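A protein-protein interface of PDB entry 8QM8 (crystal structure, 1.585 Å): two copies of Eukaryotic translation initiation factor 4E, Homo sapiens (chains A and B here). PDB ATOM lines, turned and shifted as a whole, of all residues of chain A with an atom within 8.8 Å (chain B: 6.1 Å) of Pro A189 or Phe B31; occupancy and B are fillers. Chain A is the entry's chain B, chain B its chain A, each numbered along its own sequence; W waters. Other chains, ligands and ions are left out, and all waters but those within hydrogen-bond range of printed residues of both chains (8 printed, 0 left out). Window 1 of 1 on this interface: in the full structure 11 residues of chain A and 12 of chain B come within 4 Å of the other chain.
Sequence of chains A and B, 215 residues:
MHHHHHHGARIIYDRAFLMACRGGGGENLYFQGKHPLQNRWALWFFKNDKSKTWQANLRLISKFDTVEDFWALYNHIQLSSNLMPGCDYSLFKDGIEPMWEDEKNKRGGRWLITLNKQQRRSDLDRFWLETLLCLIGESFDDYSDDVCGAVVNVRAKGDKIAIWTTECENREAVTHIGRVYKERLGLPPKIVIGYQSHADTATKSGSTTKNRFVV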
ATOM      1  N   TRP A 111     -25.964  17.698 -18.415  1.00  0.00           N
ATOM      2  CA  TRP A 111     -25.259  16.621 -19.128  1.00  0.00           C
ATOM      3  C   TRP A 111     -26.010  15.361 -18.823  1.00  0.00           C
ATOM      4  O   TRP A 111     -26.127  15.009 -17.647  1.00  0.00           O
ATOM      5  CB  TRP A 111     -23.822  16.449 -18.638  1.00  0.00           C
ATOM      6  CG  TRP A 111     -22.927  17.501 -19.188  1.00  0.00           C
ATOM      7  CD1 TRP A 111     -22.416  18.589 -18.538  1.00  0.00           C
ATOM      8  CD2 TRP A 111     -22.456  17.579 -20.548  1.00  0.00           C
ATOM      9  NE1 TRP A 111     -21.655  19.334 -19.392  1.00  0.00           N
ATOM     10  CE2 TRP A 111     -21.673  18.738 -20.646  1.00  0.00           C
ATOM     11  CE3 TRP A 111     -22.581  16.745 -21.668  1.00  0.00           C
ATOM     12  CZ2 TRP A 111     -21.020  19.091 -21.822  1.00  0.00           C
ATOM     13  CZ3 TRP A 111     -21.955  17.122 -22.842  1.00  0.00           C
ATOM     14  CH2 TRP A 111     -21.148  18.247 -22.887  1.00  0.00           C
ATOM     15  N   ARG A 179     -16.521  16.918 -20.276  1.00  0.00           N
ATOM     16  CA  ARG A 179     -15.333  16.097 -20.573  1.00  0.00           C
ATOM     17  C   ARG A 179     -14.860  15.275 -19.366  1.00  0.00           C
ATOM     18  O   ARG A 179     -14.645  14.060 -19.441  1.00  0.00           O
ATOM     19  CB  ARG A 179     -14.244  16.988 -21.133  1.00  0.00           C
ATOM     20  CG  ARG A 179     -14.565  17.539 -22.490  1.00  0.00           C
ATOM     21  CD  ARG A 179     -13.321  18.091 -23.063  1.00  0.00           C
ATOM     22  NE  ARG A 179     -13.513  19.019 -24.183  1.00  0.00           N
ATOM     23  CZ  ARG A 179     -13.873  18.685 -25.420  1.00  0.00           C
ATOM     24  NH1 ARG A 179     -13.988  19.615 -26.354  1.00  0.00           N
ATOM     25  NH2 ARG A 179     -14.148  17.421 -25.728  1.00  0.00           N
ATOM     26  N   LYS A 182     -17.508  12.483 -18.423  1.00  0.00           N
ATOM     27  CA  LYS A 182     -17.309  11.348 -19.337  1.00  0.00           C
ATOM     28  C   LYS A 182     -16.039  10.540 -18.944  1.00  0.00           C
ATOM     29  O   LYS A 182     -16.095   9.308 -18.910  1.00  0.00           O
ATOM     30  CB  LYS A 182     -17.222  11.840 -20.756  1.00  0.00           C
ATOM     31  CG  LYS A 182     -17.035  10.744 -21.773  1.00  0.00           C
ATOM     32  CD  LYS A 182     -17.443  11.130 -23.127  1.00  0.00           C
ATOM     33  CE  LYS A 182     -16.883  10.156 -24.168  1.00  0.00           C
ATOM     34  NZ  LYS A 182     -17.344  10.531 -25.516  1.00  0.00           N
ATOM     35  N   GLU A 183     -14.926  11.217 -18.696  1.00  0.00           N
ATOM     36  CA  GLU A 183     -13.646  10.583 -18.282  1.00  0.00           C
ATOM     37  C   GLU A 183     -13.818   9.800 -17.001  1.00  0.00           C
ATOM     38  O   GLU A 183     -13.419   8.652 -16.903  1.00  0.00           O
ATOM     39  CB  GLU A 183     -12.609  11.720 -18.213  1.00  0.00           C
ATOM     40  CG  GLU A 183     -11.305  11.518 -17.573  1.00  0.00           C
ATOM     41  CD  GLU A 183     -10.720  12.908 -17.336  1.00  0.00           C
ATOM     42  OE1 GLU A 183     -10.088  13.044 -16.278  1.00  0.00           O
ATOM     43  OE2 GLU A 183     -10.867  13.824 -18.179  1.00  0.00           O
ATOM     44  N   GLY A 186     -15.761   6.705 -17.315  1.00  0.00           N
ATOM     45  CA  GLY A 186     -15.007   5.688 -18.024  1.00  0.00           C
ATOM     46  C   GLY A 186     -15.645   5.303 -19.325  1.00  0.00           C
ATOM     47  O   GLY A 186     -15.444   4.178 -19.772  1.00  0.00           O
ATOM     48  N   LEU A 187     -16.421   6.201 -19.942  1.00  0.00           N
ATOM     49  CA  LEU A 187     -17.140   5.858 -21.159  1.00  0.00           C
ATOM     50  C   LEU A 187     -16.133   5.810 -22.290  1.00  0.00           C
ATOM     51  O   LEU A 187     -15.246   6.659 -22.375  1.00  0.00           O
ATOM     52  CB  LEU A 187     -18.199   6.872 -21.543  1.00  0.00           C
ATOM     53  CG  LEU A 187     -19.317   7.134 -20.520  1.00  0.00           C
ATOM     54  CD1 LEU A 187     -20.313   8.195 -21.026  1.00  0.00           C
ATOM     55  CD2 LEU A 187     -20.105   5.888 -20.232  1.00  0.00           C
ATOM     56  N   PRO A 188     -16.267   4.829 -23.163  1.00  0.00           N
ATOM     57  CA  PRO A 188     -15.464   4.830 -24.378  1.00  0.00           C
ATOM     58  C   PRO A 188     -15.617   6.142 -25.166  1.00  0.00           C
ATOM     59  O   PRO A 188     -16.687   6.707 -25.175  1.00  0.00           O
ATOM     60  CB  PRO A 188     -16.037   3.648 -25.160  1.00  0.00           C
ATOM     61  CG  PRO A 188     -16.593   2.720 -24.103  1.00  0.00           C
ATOM     62  CD  PRO A 188     -17.154   3.640 -23.091  1.00  0.00           C
ATOM     63  N   PRO A 189     -14.556   6.621 -25.815  1.00  0.00           N
ATOM     64  CA  PRO A 189     -14.693   7.852 -26.647  1.00  0.00           C
ATOM     65  C   PRO A 189     -15.877   7.887 -27.584  1.00  0.00           C
ATOM     66  O   PRO A 189     -16.510   8.949 -27.745  1.00  0.00           O
ATOM     67  CB  PRO A 189     -13.368   7.891 -27.387  1.00  0.00           C
ATOM     68  CG  PRO A 189     -12.397   7.227 -26.414  1.00  0.00           C
ATOM     69  CD  PRO A 189     -13.177   6.106 -25.853  1.00  0.00           C
ATOM     70  N   LYS A 190     -16.225   6.751 -28.209  1.00  0.00           N
ATOM     71  CA  LYS A 190     -17.302   6.730 -29.180  1.00  0.00           C
ATOM     72  C   LYS A 190     -18.725   6.910 -28.613  1.00  0.00           C
ATOM     73  O   LYS A 190     -19.651   7.172 -29.387  1.00  0.00           O
ATOM     74  CB  LYS A 190     -17.264   5.430 -29.994  1.00  0.00           C
ATOM     75  CG  LYS A 190     -17.633   4.207 -29.141  1.00  0.00           C
ATOM     76  CD  LYS A 190     -17.535   2.855 -29.884  1.00  0.00           C
ATOM     77  CE  LYS A 190     -18.530   2.756 -30.982  1.00  0.00           C
ATOM     78  NZ  LYS A 190     -18.574   1.385 -31.612  1.00  0.00           N
ATOM     79  N   ILE A 191     -18.885   6.770 -27.306  1.00  0.00           N
ATOM     80  CA  ILE A 191     -20.156   6.971 -26.623  1.00  0.00           C
ATOM     81  C   ILE A 191     -20.305   8.425 -26.303  1.00  0.00           C
ATOM     82  O   ILE A 191     -19.762   8.897 -25.339  1.00  0.00           O
ATOM     83  CB  ILE A 191     -20.276   6.104 -25.350  1.00  0.00           C
ATOM     84  CG1 ILE A 191     -20.092   4.598 -25.662  1.00  0.00           C
ATOM     85  CG2 ILE A 191     -21.666   6.343 -24.658  1.00  0.00           C
ATOM     86  CD1 ILE A 191     -20.977   4.046 -26.638  1.00  0.00           C
ATOM     87  N   VAL A 192     -21.034   9.129 -27.132  1.00  0.00           N
ATOM     88  CA  VAL A 192     -21.210  10.576 -27.070  1.00  0.00           C
ATOM     89  C   VAL A 192     -22.241  10.900 -25.992  1.00  0.00           C
ATOM     90  O   VAL A 192     -23.271  10.244 -25.928  1.00  0.00           O
ATOM     91  CB  VAL A 192     -21.659  11.081 -28.472  1.00  0.00           C
ATOM     92  CG1 VAL A 192     -22.056  12.534 -28.438  1.00  0.00           C
ATOM     93  CG2 VAL A 192     -20.553  10.837 -29.503  1.00  0.00           C
ATOM     94  N   ILE A 193     -21.950  11.879 -25.130  1.00  0.00           N
ATOM     95  CA  ILE A 193     -22.940  12.409 -24.199  1.00  0.00           C
ATOM     96  C   ILE A 193     -23.234  13.864 -24.570  1.00  0.00           C
ATOM     97  O   ILE A 193     -22.380  14.543 -25.074  1.00  0.00           O
ATOM     98  CB  ILE A 193     -22.509  12.264 -22.739  1.00  0.00           C
ATOM     99  CG1 ILE A 193     -21.344  13.227 -22.337  1.00  0.00           C
ATOM    100  CG2 ILE A 193     -22.188  10.810 -22.449  1.00  0.00           C
ATOM    101  CD1 ILE A 193     -21.073  13.339 -20.965  1.00  0.00           C
ATOM    102  N   GLY A 194     -24.457  14.322 -24.292  1.00  0.00           N
ATOM    103  CA  GLY A 194     -24.929  15.620 -24.721  1.00  0.00           C
ATOM    104  C   GLY A 194     -25.427  16.505 -23.604  1.00  0.00           C
ATOM    105  O   GLY A 194     -25.924  15.997 -22.584  1.00  0.00           O
ATOM    106  N   THR A 209     -27.483  13.525 -29.416  1.00  0.00           N
ATOM    107  CA  THR A 209     -26.605  13.490 -30.584  1.00  0.00           C
ATOM    108  C   THR A 209     -26.558  14.853 -31.275  1.00  0.00           C
ATOM    109  O   THR A 209     -25.479  15.297 -31.670  1.00  0.00           O
ATOM    110  CB  THR A 209     -27.008  12.351 -31.517  1.00  0.00           C
ATOM    111  OG1 THR A 209     -26.127  12.344 -32.660  1.00  0.00           O
ATOM    112  CG2 THR A 209     -28.463  12.443 -31.969  1.00  0.00           C
ATOM    113  N   LYS A 210     -27.736  15.519 -31.422  1.00  0.00           N
ATOM    114  CA  LYS A 210     -27.832  16.866 -31.968  1.00  0.00           C
ATOM    115  C   LYS A 210     -27.797  17.992 -30.905  1.00  0.00           C
ATOM    116  O   LYS A 210     -27.974  19.156 -31.259  1.00  0.00           O
ATOM    117  CB  LYS A 210     -29.101  17.004 -32.830  1.00  0.00           C
ATOM    118  CG  LYS A 210     -30.426  17.110 -32.086  1.00  0.00           C
ATOM    119  CD  LYS A 210     -31.568  16.905 -33.090  1.00  0.00           C
ATOM    120  CE  LYS A 210     -32.880  17.545 -32.668  1.00  0.00           C
ATOM    121  NZ  LYS A 210     -33.894  17.487 -33.766  1.00  0.00           N
ATOM    122  N   PHE A 213     -24.021  21.065 -26.749  1.00  0.00           N
ATOM    123  CA  PHE A 213     -22.639  20.566 -26.694  1.00  0.00           C
ATOM    124  C   PHE A 213     -22.666  19.022 -26.636  1.00  0.00           C
ATOM    125  O   PHE A 213     -23.537  18.416 -26.049  1.00  0.00           O
ATOM    126  CB  PHE A 213     -21.937  21.096 -25.446  1.00  0.00           C
ATOM    127  CG  PHE A 213     -22.065  22.571 -25.185  1.00  0.00           C
ATOM    128  CD1 PHE A 213     -21.260  23.478 -25.846  1.00  0.00           C
ATOM    129  CD2 PHE A 213     -22.955  23.050 -24.242  1.00  0.00           C
ATOM    130  CE1 PHE A 213     -21.373  24.847 -25.582  1.00  0.00           C
ATOM    131  CE2 PHE A 213     -23.038  24.412 -23.961  1.00  0.00           C
ATOM    132  CZ  PHE A 213     -22.258  25.299 -24.640  1.00  0.00           C
ATOM    133  N   VAL A 214     -21.690  18.386 -27.252  1.00  0.00           N
ATOM    134  CA  VAL A 214     -21.477  16.958 -27.173  1.00  0.00           C
ATOM    135  C   VAL A 214     -20.004  16.719 -26.887  1.00  0.00           C
ATOM    136  O   VAL A 214     -19.154  17.470 -27.394  1.00  0.00           O
ATOM    137  CB  VAL A 214     -21.935  16.210 -28.448  1.00  0.00           C
ATOM    138  CG1 VAL A 214     -23.436  16.399 -28.707  1.00  0.00           C
ATOM    139  CG2 VAL A 214     -21.112  16.603 -29.646  1.00  0.00           C
ATOM    140  N   VAL A 215     -19.697  15.704 -26.093  1.00  0.00           N
ATOM    141  CA  VAL A 215     -18.338  15.243 -25.830  1.00  0.00           C
ATOM    142  C   VAL A 215     -18.275  13.737 -25.799  1.00  0.00           C
ATOM    143  O   VAL A 215     -17.131  13.199 -25.784  1.00  0.00           O
ATOM    144  CB  VAL A 215     -17.715  15.798 -24.522  1.00  0.00           C
ATOM    145  CG1 VAL A 215     -17.629  17.317 -24.579  1.00  0.00           C
ATOM    146  CG2 VAL A 215     -18.501  15.320 -23.289  1.00  0.00           C
ATOM    147  OXT VAL A 215     -19.346  13.122 -25.758  1.00  0.00           O
ATOM    148  N   ASN B  28     -16.819  13.417 -40.102  1.00  0.00           N
ATOM    149  CA  ASN B  28     -17.352  12.104 -39.764  1.00  0.00           C
ATOM    150  C   ASN B  28     -18.867  12.119 -39.849  1.00  0.00           C
ATOM    151  O   ASN B  28     -19.507  13.165 -39.699  1.00  0.00           O
ATOM    152  CB  ASN B  28     -16.966  11.672 -38.352  1.00  0.00           C
ATOM    153  CG  ASN B  28     -17.085  10.183 -38.107  1.00  0.00           C
ATOM    154  OD1 ASN B  28     -17.137   9.377 -39.025  1.00  0.00           O
ATOM    155  ND2 ASN B  28     -17.117   9.785 -36.856  1.00  0.00           N
ATOM    156  N   LEU B  29     -19.421  10.960 -40.100  1.00  0.00           N
ATOM    157  CA  LEU B  29     -20.855  10.774 -40.242  1.00  0.00           C
ATOM    158  C   LEU B  29     -21.612  10.767 -38.889  1.00  0.00           C
ATOM    159  O   LEU B  29     -22.849  10.747 -38.879  1.00  0.00           O
ATOM    160  CB  LEU B  29     -21.114   9.459 -41.006  1.00  0.00           C
ATOM    161  CG  LEU B  29     -20.477   9.288 -42.409  1.00  0.00           C
ATOM    162  CD1 LEU B  29     -20.823   7.965 -42.971  1.00  0.00           C
ATOM    163  CD2 LEU B  29     -21.000  10.314 -43.425  1.00  0.00           C
ATOM    164  N   TYR B  30     -20.895  10.793 -37.755  1.00  0.00           N
ATOM    165  CA  TYR B  30     -21.542  10.999 -36.463  1.00  0.00           C
ATOM    166  C   TYR B  30     -20.643  11.824 -35.550  1.00  0.00           C
ATOM    167  O   TYR B  30     -19.604  12.314 -36.017  1.00  0.00           O
ATOM    168  CB  TYR B  30     -21.996   9.657 -35.855  1.00  0.00           C
ATOM    169  CG  TYR B  30     -20.897   8.788 -35.279  1.00  0.00           C
ATOM    170  CD1 TYR B  30     -19.976   8.161 -36.104  1.00  0.00           C
ATOM    171  CD2 TYR B  30     -20.813   8.554 -33.915  1.00  0.00           C
ATOM    172  CE1 TYR B  30     -18.985   7.333 -35.583  1.00  0.00           C
ATOM    173  CE2 TYR B  30     -19.816   7.746 -33.381  1.00  0.00           C
ATOM    174  CZ  TYR B  30     -18.905   7.133 -34.218  1.00  0.00           C
ATOM    175  OH  TYR B  30     -17.950   6.301 -33.670  1.00  0.00           O
ATOM    176  N   PHE B  31     -21.039  12.025 -34.279  1.00  0.00           N
ATOM    177  CA  PHE B  31     -20.231  12.751 -33.301  1.00  0.00           C
ATOM    178  C   PHE B  31     -20.071  14.218 -33.701  1.00  0.00           C
ATOM    179  O   PHE B  31     -19.063  14.869 -33.376  1.00  0.00           O
ATOM    180  CB  PHE B  31     -18.866  12.095 -33.081  1.00  0.00           C
ATOM    181  CG  PHE B  31     -18.241  12.274 -31.692  1.00  0.00           C
ATOM    182  CD1 PHE B  31     -18.570  13.369 -30.890  1.00  0.00           C
ATOM    183  CD2 PHE B  31     -17.339  11.343 -31.194  1.00  0.00           C
ATOM    184  CE1 PHE B  31     -17.993  13.527 -29.615  1.00  0.00           C
ATOM    185  CE2 PHE B  31     -16.745  11.517 -29.920  1.00  0.00           C
ATOM    186  CZ  PHE B  31     -17.101  12.600 -29.148  1.00  0.00           C
ATOM    187  N   GLN B  32     -21.094  14.774 -34.392  1.00  0.00           N
ATOM    188  CA  GLN B  32     -21.026  16.095 -34.988  1.00  0.00           C
ATOM    189  C   GLN B  32     -19.738  16.300 -35.802  1.00  0.00           C
ATOM    190  O   GLN B  32     -19.176  17.386 -35.813  1.00  0.00           O
ATOM    191  CB  GLN B  32     -21.252  17.162 -33.895  1.00  0.00           C
ATOM    192  CG  GLN B  32     -22.615  17.003 -33.222  1.00  0.00           C
ATOM    193  CD  GLN B  32     -22.988  18.155 -32.324  1.00  0.00           C
ATOM    194  OE1 GLN B  32     -22.272  19.151 -32.212  1.00  0.00           O
ATOM    195  NE2 GLN B  32     -24.134  18.048 -31.664  1.00  0.00           N
ATOM    196  N   GLY B  33     -19.318  15.237 -36.477  1.00  0.00           N
ATOM    197  CA  GLY B  33     -18.170  15.234 -37.373  1.00  0.00           C
ATOM    198  C   GLY B  33     -16.860  14.719 -36.802  1.00  0.00           C
ATOM    199  O   GLY B  33     -15.927  14.480 -37.589  1.00  0.00           O
ATOM    200  N   LYS B  34     -16.742  14.540 -35.451  1.00  0.00           N
ATOM    201  CA  LYS B  34     -15.458  14.062 -34.894  1.00  0.00           C
ATOM    202  C   LYS B  34     -15.316  12.537 -34.997  1.00  0.00           C
ATOM    203  O   LYS B  34     -16.285  11.816 -34.874  1.00  0.00           O
ATOM    204  CB  LYS B  34     -15.230  14.580 -33.466  1.00  0.00           C
ATOM    205  CG  LYS B  34     -14.970  16.095 -33.433  1.00  0.00           C
ATOM    206  CD  LYS B  34     -14.658  16.571 -32.079  1.00  0.00           C
ATOM    207  CE  LYS B  34     -14.767  18.068 -31.969  1.00  0.00           C
ATOM    208  NZ  LYS B  34     -13.955  18.774 -32.994  1.00  0.00           N
ATOM    209  N   HIS B  35     -14.102  12.052 -35.214  1.00  0.00           N
ATOM    210  CA  HIS B  35     -13.791  10.652 -35.342  1.00  0.00           C
ATOM    211  C   HIS B  35     -13.291  10.197 -33.958  1.00  0.00           C
ATOM    212  O   HIS B  35     -12.206  10.621 -33.553  1.00  0.00           O
ATOM    213  CB  HIS B  35     -12.678  10.440 -36.402  1.00  0.00           C
ATOM    214  CG  HIS B  35     -13.130  10.763 -37.782  1.00  0.00           C
ATOM    215  ND1 HIS B  35     -13.097  12.036 -38.266  1.00  0.00           N
ATOM    216  CD2 HIS B  35     -13.610   9.936 -38.747  1.00  0.00           C
ATOM    217  CE1 HIS B  35     -13.581  11.987 -39.502  1.00  0.00           C
ATOM    218  NE2 HIS B  35     -13.920  10.755 -39.843  1.00  0.00           N
ATOM    219  N   PRO B  36     -14.056   9.391 -33.233  1.00  0.00           N
ATOM    220  CA  PRO B  36     -13.575   8.946 -31.911  1.00  0.00           C
ATOM    221  C   PRO B  36     -12.429   7.978 -31.987  1.00  0.00           C
ATOM    222  O   PRO B  36     -12.336   7.213 -32.903  1.00  0.00           O
ATOM    223  CB  PRO B  36     -14.777   8.259 -31.338  1.00  0.00           C
ATOM    224  CG  PRO B  36     -15.505   7.751 -32.511  1.00  0.00           C
ATOM    225  CD  PRO B  36     -15.373   8.811 -33.528  1.00  0.00           C
ATOM    226  N   LEU B  37     -11.557   8.023 -31.010  1.00  0.00           N
ATOM    227  CA  LEU B  37     -10.464   7.076 -30.896  1.00  0.00           C
ATOM    228  C   LEU B  37     -10.900   5.879 -30.102  1.00  0.00           C
ATOM    229  O   LEU B  37     -11.896   5.938 -29.372  1.00  0.00           O
ATOM    230  CB  LEU B  37      -9.312   7.766 -30.189  1.00  0.00           C
ATOM    231  CG  LEU B  37      -8.664   8.995 -30.877  1.00  0.00           C
ATOM    232  CD1 LEU B  37      -7.605   9.564 -29.991  1.00  0.00           C
ATOM    233  CD2 LEU B  37      -8.083   8.627 -32.240  1.00  0.00           C
ATOM    234  N   GLN B  38     -10.168   4.793 -30.216  1.00  0.00           N
ATOM    235  CA  GLN B  38     -10.382   3.635 -29.354  1.00  0.00           C
ATOM    236  C   GLN B  38     -10.221   3.935 -27.902  1.00  0.00           C
ATOM    237  O   GLN B  38     -10.982   3.431 -27.062  1.00  0.00           O
ATOM    238  CB  GLN B  38      -9.475   2.514 -29.770  1.00  0.00           C
ATOM    239  CG  GLN B  38      -9.579   1.274 -28.926  1.00  0.00           C
ATOM    240  CD  GLN B  38     -10.888   0.583 -29.088  1.00  0.00           C
ATOM    241  OE1 GLN B  38     -11.594   0.738 -30.092  1.00  0.00           O
ATOM    242  NE2 GLN B  38     -11.257  -0.172 -28.092  1.00  0.00           N
ATOM    243  N   ASN B  39      -9.199   4.719 -27.595  1.00  0.00           N
ATOM    244  CA  ASN B  39      -8.814   5.077 -26.250  1.00  0.00           C
ATOM    245  C   ASN B  39      -8.773   6.556 -26.071  1.00  0.00           C
ATOM    246  O   ASN B  39      -8.575   7.304 -27.001  1.00  0.00           O
ATOM    247  CB  ASN B  39      -7.445   4.518 -25.879  1.00  0.00           C
ATOM    248  CG  ASN B  39      -7.508   3.068 -25.636  1.00  0.00           C
ATOM    249  OD1 ASN B  39      -8.054   2.650 -24.630  1.00  0.00           O
ATOM    250  ND2 ASN B  39      -7.019   2.240 -26.547  1.00  0.00           N
ATOM    251  N   ARG B  40      -8.978   6.987 -24.827  1.00  0.00           N
ATOM    252  CA  ARG B  40      -8.698   8.328 -24.394  1.00  0.00           C
ATOM    253  C   ARG B  40      -7.242   8.416 -23.948  1.00  0.00           C
ATOM    254  O   ARG B  40      -6.719   7.506 -23.280  1.00  0.00           O
ATOM    255  CB  ARG B  40      -9.638   8.682 -23.220  1.00  0.00           C
ATOM    256  CG  ARG B  40      -9.552  10.072 -22.613  1.00  0.00           C
ATOM    257  CD  ARG B  40     -10.701  10.284 -21.544  1.00  0.00           C
ATOM    258  NE  ARG B  40     -11.914  10.127 -22.292  1.00  0.00           N
ATOM    259  CZ  ARG B  40     -12.793   9.123 -22.228  1.00  0.00           C
ATOM    260  NH1 ARG B  40     -12.667   8.167 -21.318  1.00  0.00           N
ATOM    261  NH2 ARG B  40     -13.800   9.079 -23.062  1.00  0.00           N
ATOM    262  N   ASP B  65      -9.819  12.467 -26.980  1.00  0.00           N
ATOM    263  CA  ASP B  65     -10.342  11.158 -27.371  1.00  0.00           C
ATOM    264  C   ASP B  65     -10.945  11.129 -28.785  1.00  0.00           C
ATOM    265  O   ASP B  65     -11.669  10.188 -29.115  1.00  0.00           O
ATOM    266  CB  ASP B  65     -11.314  10.650 -26.310  1.00  0.00           C
ATOM    267  CG  ASP B  65     -12.622  11.415 -26.188  1.00  0.00           C
ATOM    268  OD1 ASP B  65     -12.820  12.338 -26.950  1.00  0.00           O
ATOM    269  OD2 ASP B  65     -13.446  11.082 -25.275  1.00  0.00           O
ATOM    270  N   THR B  66     -10.610  12.148 -29.631  1.00  0.00           N
ATOM    271  CA  THR B  66     -10.943  12.148 -31.020  1.00  0.00           C
ATOM    272  C   THR B  66      -9.711  12.501 -31.871  1.00  0.00           C
ATOM    273  O   THR B  66      -8.770  13.157 -31.420  1.00  0.00           O
ATOM    274  CB  THR B  66     -12.097  13.126 -31.341  1.00  0.00           C
ATOM    275  OG1 THR B  66     -11.655  14.450 -31.263  1.00  0.00           O
ATOM    276  CG2 THR B  66     -13.372  12.906 -30.449  1.00  0.00           C
HETATM  277  O   HOH W   1     -13.826  12.828 -21.718  1.00  0.00           O
HETATM  278  O   HOH W   2     -26.262  20.661 -32.127  1.00  0.00           O
HETATM  279  O   HOH W   3     -23.373  11.286 -32.565  1.00  0.00           O
HETATM  280  O   HOH W   4     -23.130  13.709 -32.134  1.00  0.00           O
HETATM  281  O   HOH W   5     -15.016  13.826 -27.264  1.00  0.00           O
HETATM  282  O   HOH W   6     -11.568   7.691 -18.767  1.00  0.00           O
HETATM  283  O   HOH W   7     -14.284   4.667 -28.612  1.00  0.00           O
HETATM  284  O   HOH W   8     -14.750  13.098 -24.211  1.00  0.00           O
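Of the printed residues of chain B, Lys A182 touches Arg B40 (3.4 Å) and Asp B65 (3.7 Å).
Pro A189 touches just these residues of chain B: Phe B31 (3.4 Å), Pro B36 (3.9 Å), Leu B37 (3.1 Å), Gln B38 (3.7 Å), Asn B39 (3.7 Å), Arg B40 (3.8 Å) and Asp B65 (3.3 Å).
Printed residues of chain B within 4 Å of Val A192: Phe B31 (3.5 Å).
Of the printed residues of chain B, Lys A210 touches Gln B32 (3.7 Å).
Of chain A, only Pro A189 (3.4 Å), Val A192 (3.5 Å) and Val A215 (3.4 Å) come within 4 Å of Phe B31.
Of the printed residues of chain A, Arg B40 touches Lys A182, Leu A187 and Pro A189.
Among the printed residues, pairs that only touch across the chains: Lys A182 with Arg B40 (3.4 Å), Pro A189 with Phe B31 (3.4 Å), Pro A189 with Pro B36 (3.9 Å), Pro A189 with Leu B37 (3.1 Å), Pro A189 with Gln B38 (3.7 Å), Pro A189 with Asn B39 (3.7 Å), Pro A189 with Arg B40 (3.8 Å), Pro A189 with Asp B65 (3.3 Å), Lys A190 with Tyr B30 (3.8 Å), Lys A190 with Pro B36 (3.7 Å), Val A192 with Phe B31 (3.5 Å), Lys A210 with Gln B32 (3.7 Å), Val A214 with Gln B32 (3.5 Å) and Val A215 with Phe B31 (3.4 Å).
Water W2 bridges O of Lys A210 (2.4 Å) and NE2 of Gln B32 (3.4 Å).
Water W5 bridges O of Val A215 (2.7 Å) and OD1 of Asp B65 (2.7 Å).
Water W6 bridges the backbone carbonyl oxygen (O) of Glu A183 and the guanidinium group (NH1) of Arg B40.
Water W7 lies within hydrogen-bond range of the backbone carbonyl oxygen of Leu B37 (2.8 Å) and the backbone NH of Lys A190 (2.9 Å).
Water W4 lies within hydrogen-bond range of O of Thr A209 (2.9 Å), N of Gln B32 (3.2 Å) and N of Phe B31 (3.4 Å).
Water W3 bridges the side-chain hydroxyl of Thr A209 (3.0 Å) and the backbone NH of Phe B31 (3.0 Å).
OD2 of Asp B65 lies within salt-bridge range of NZ of Lys A182 (3.9 Å).
NE2 of Gln B32 lies within hydrogen-bond range of O of Thr A209, at 3.1 Å.
The backbone carbonyl oxygen (O) of Leu A187 sits at hydrogen-bond distance from the guanidinium group (NH2) of Arg B40, 2.9 Å away.
Of the 18 printed residues of chain A, 9 touch a printed residue of chain B.
Hydrophobic or aromatic side chains of chain A that line the printed part of chain B: Pro A189, Val A192 and Val A214.
Printed residues of chain B that touch a printed residue of chain A: Tyr B30, Phe B31, Gln B32, Pro B36, Leu B37, Gln B38, Asn B39, Arg B40 and Asp B65.
Hydrophobic or aromatic side chains of chain B within 4 Å of the printed part of chain A: Tyr B30, Phe B31 and Pro B36.
Among the printed residues, Asp or Glu carboxylates within 4 Å of a Lys or Arg side-chain nitrogen of the other chain: Lys A182 with Asp B65 (3.9 Å).
No position is printed for both chains.
The side-chain carboxylate (OD2) of Asp B65 is in salt-bridge range of the guanidinium group (NH2) of Arg B40, at 3.0 Å.
The side-chain amino group (NZ) of Lys A182 lies within hydrogen-bond range of the backbone carbonyl oxygen (O) of Pro A189 (2.9 Å).
N of Ile A193 lies within hydrogen-bond range of OXT of Val A215.
N of Leu B37 lies within hydrogen-bond range of O of Asp B65.
The side-chain amino group (NZ) of Lys A182 lies within hydrogen-bond range of the backbone carbonyl oxygen (O) of Ile A191, at 2.9 Å.
The backbone NH (N) of Leu A187 sits at hydrogen-bond distance from the backbone carbonyl oxygen (O) of Lys A182 (3.3 Å).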
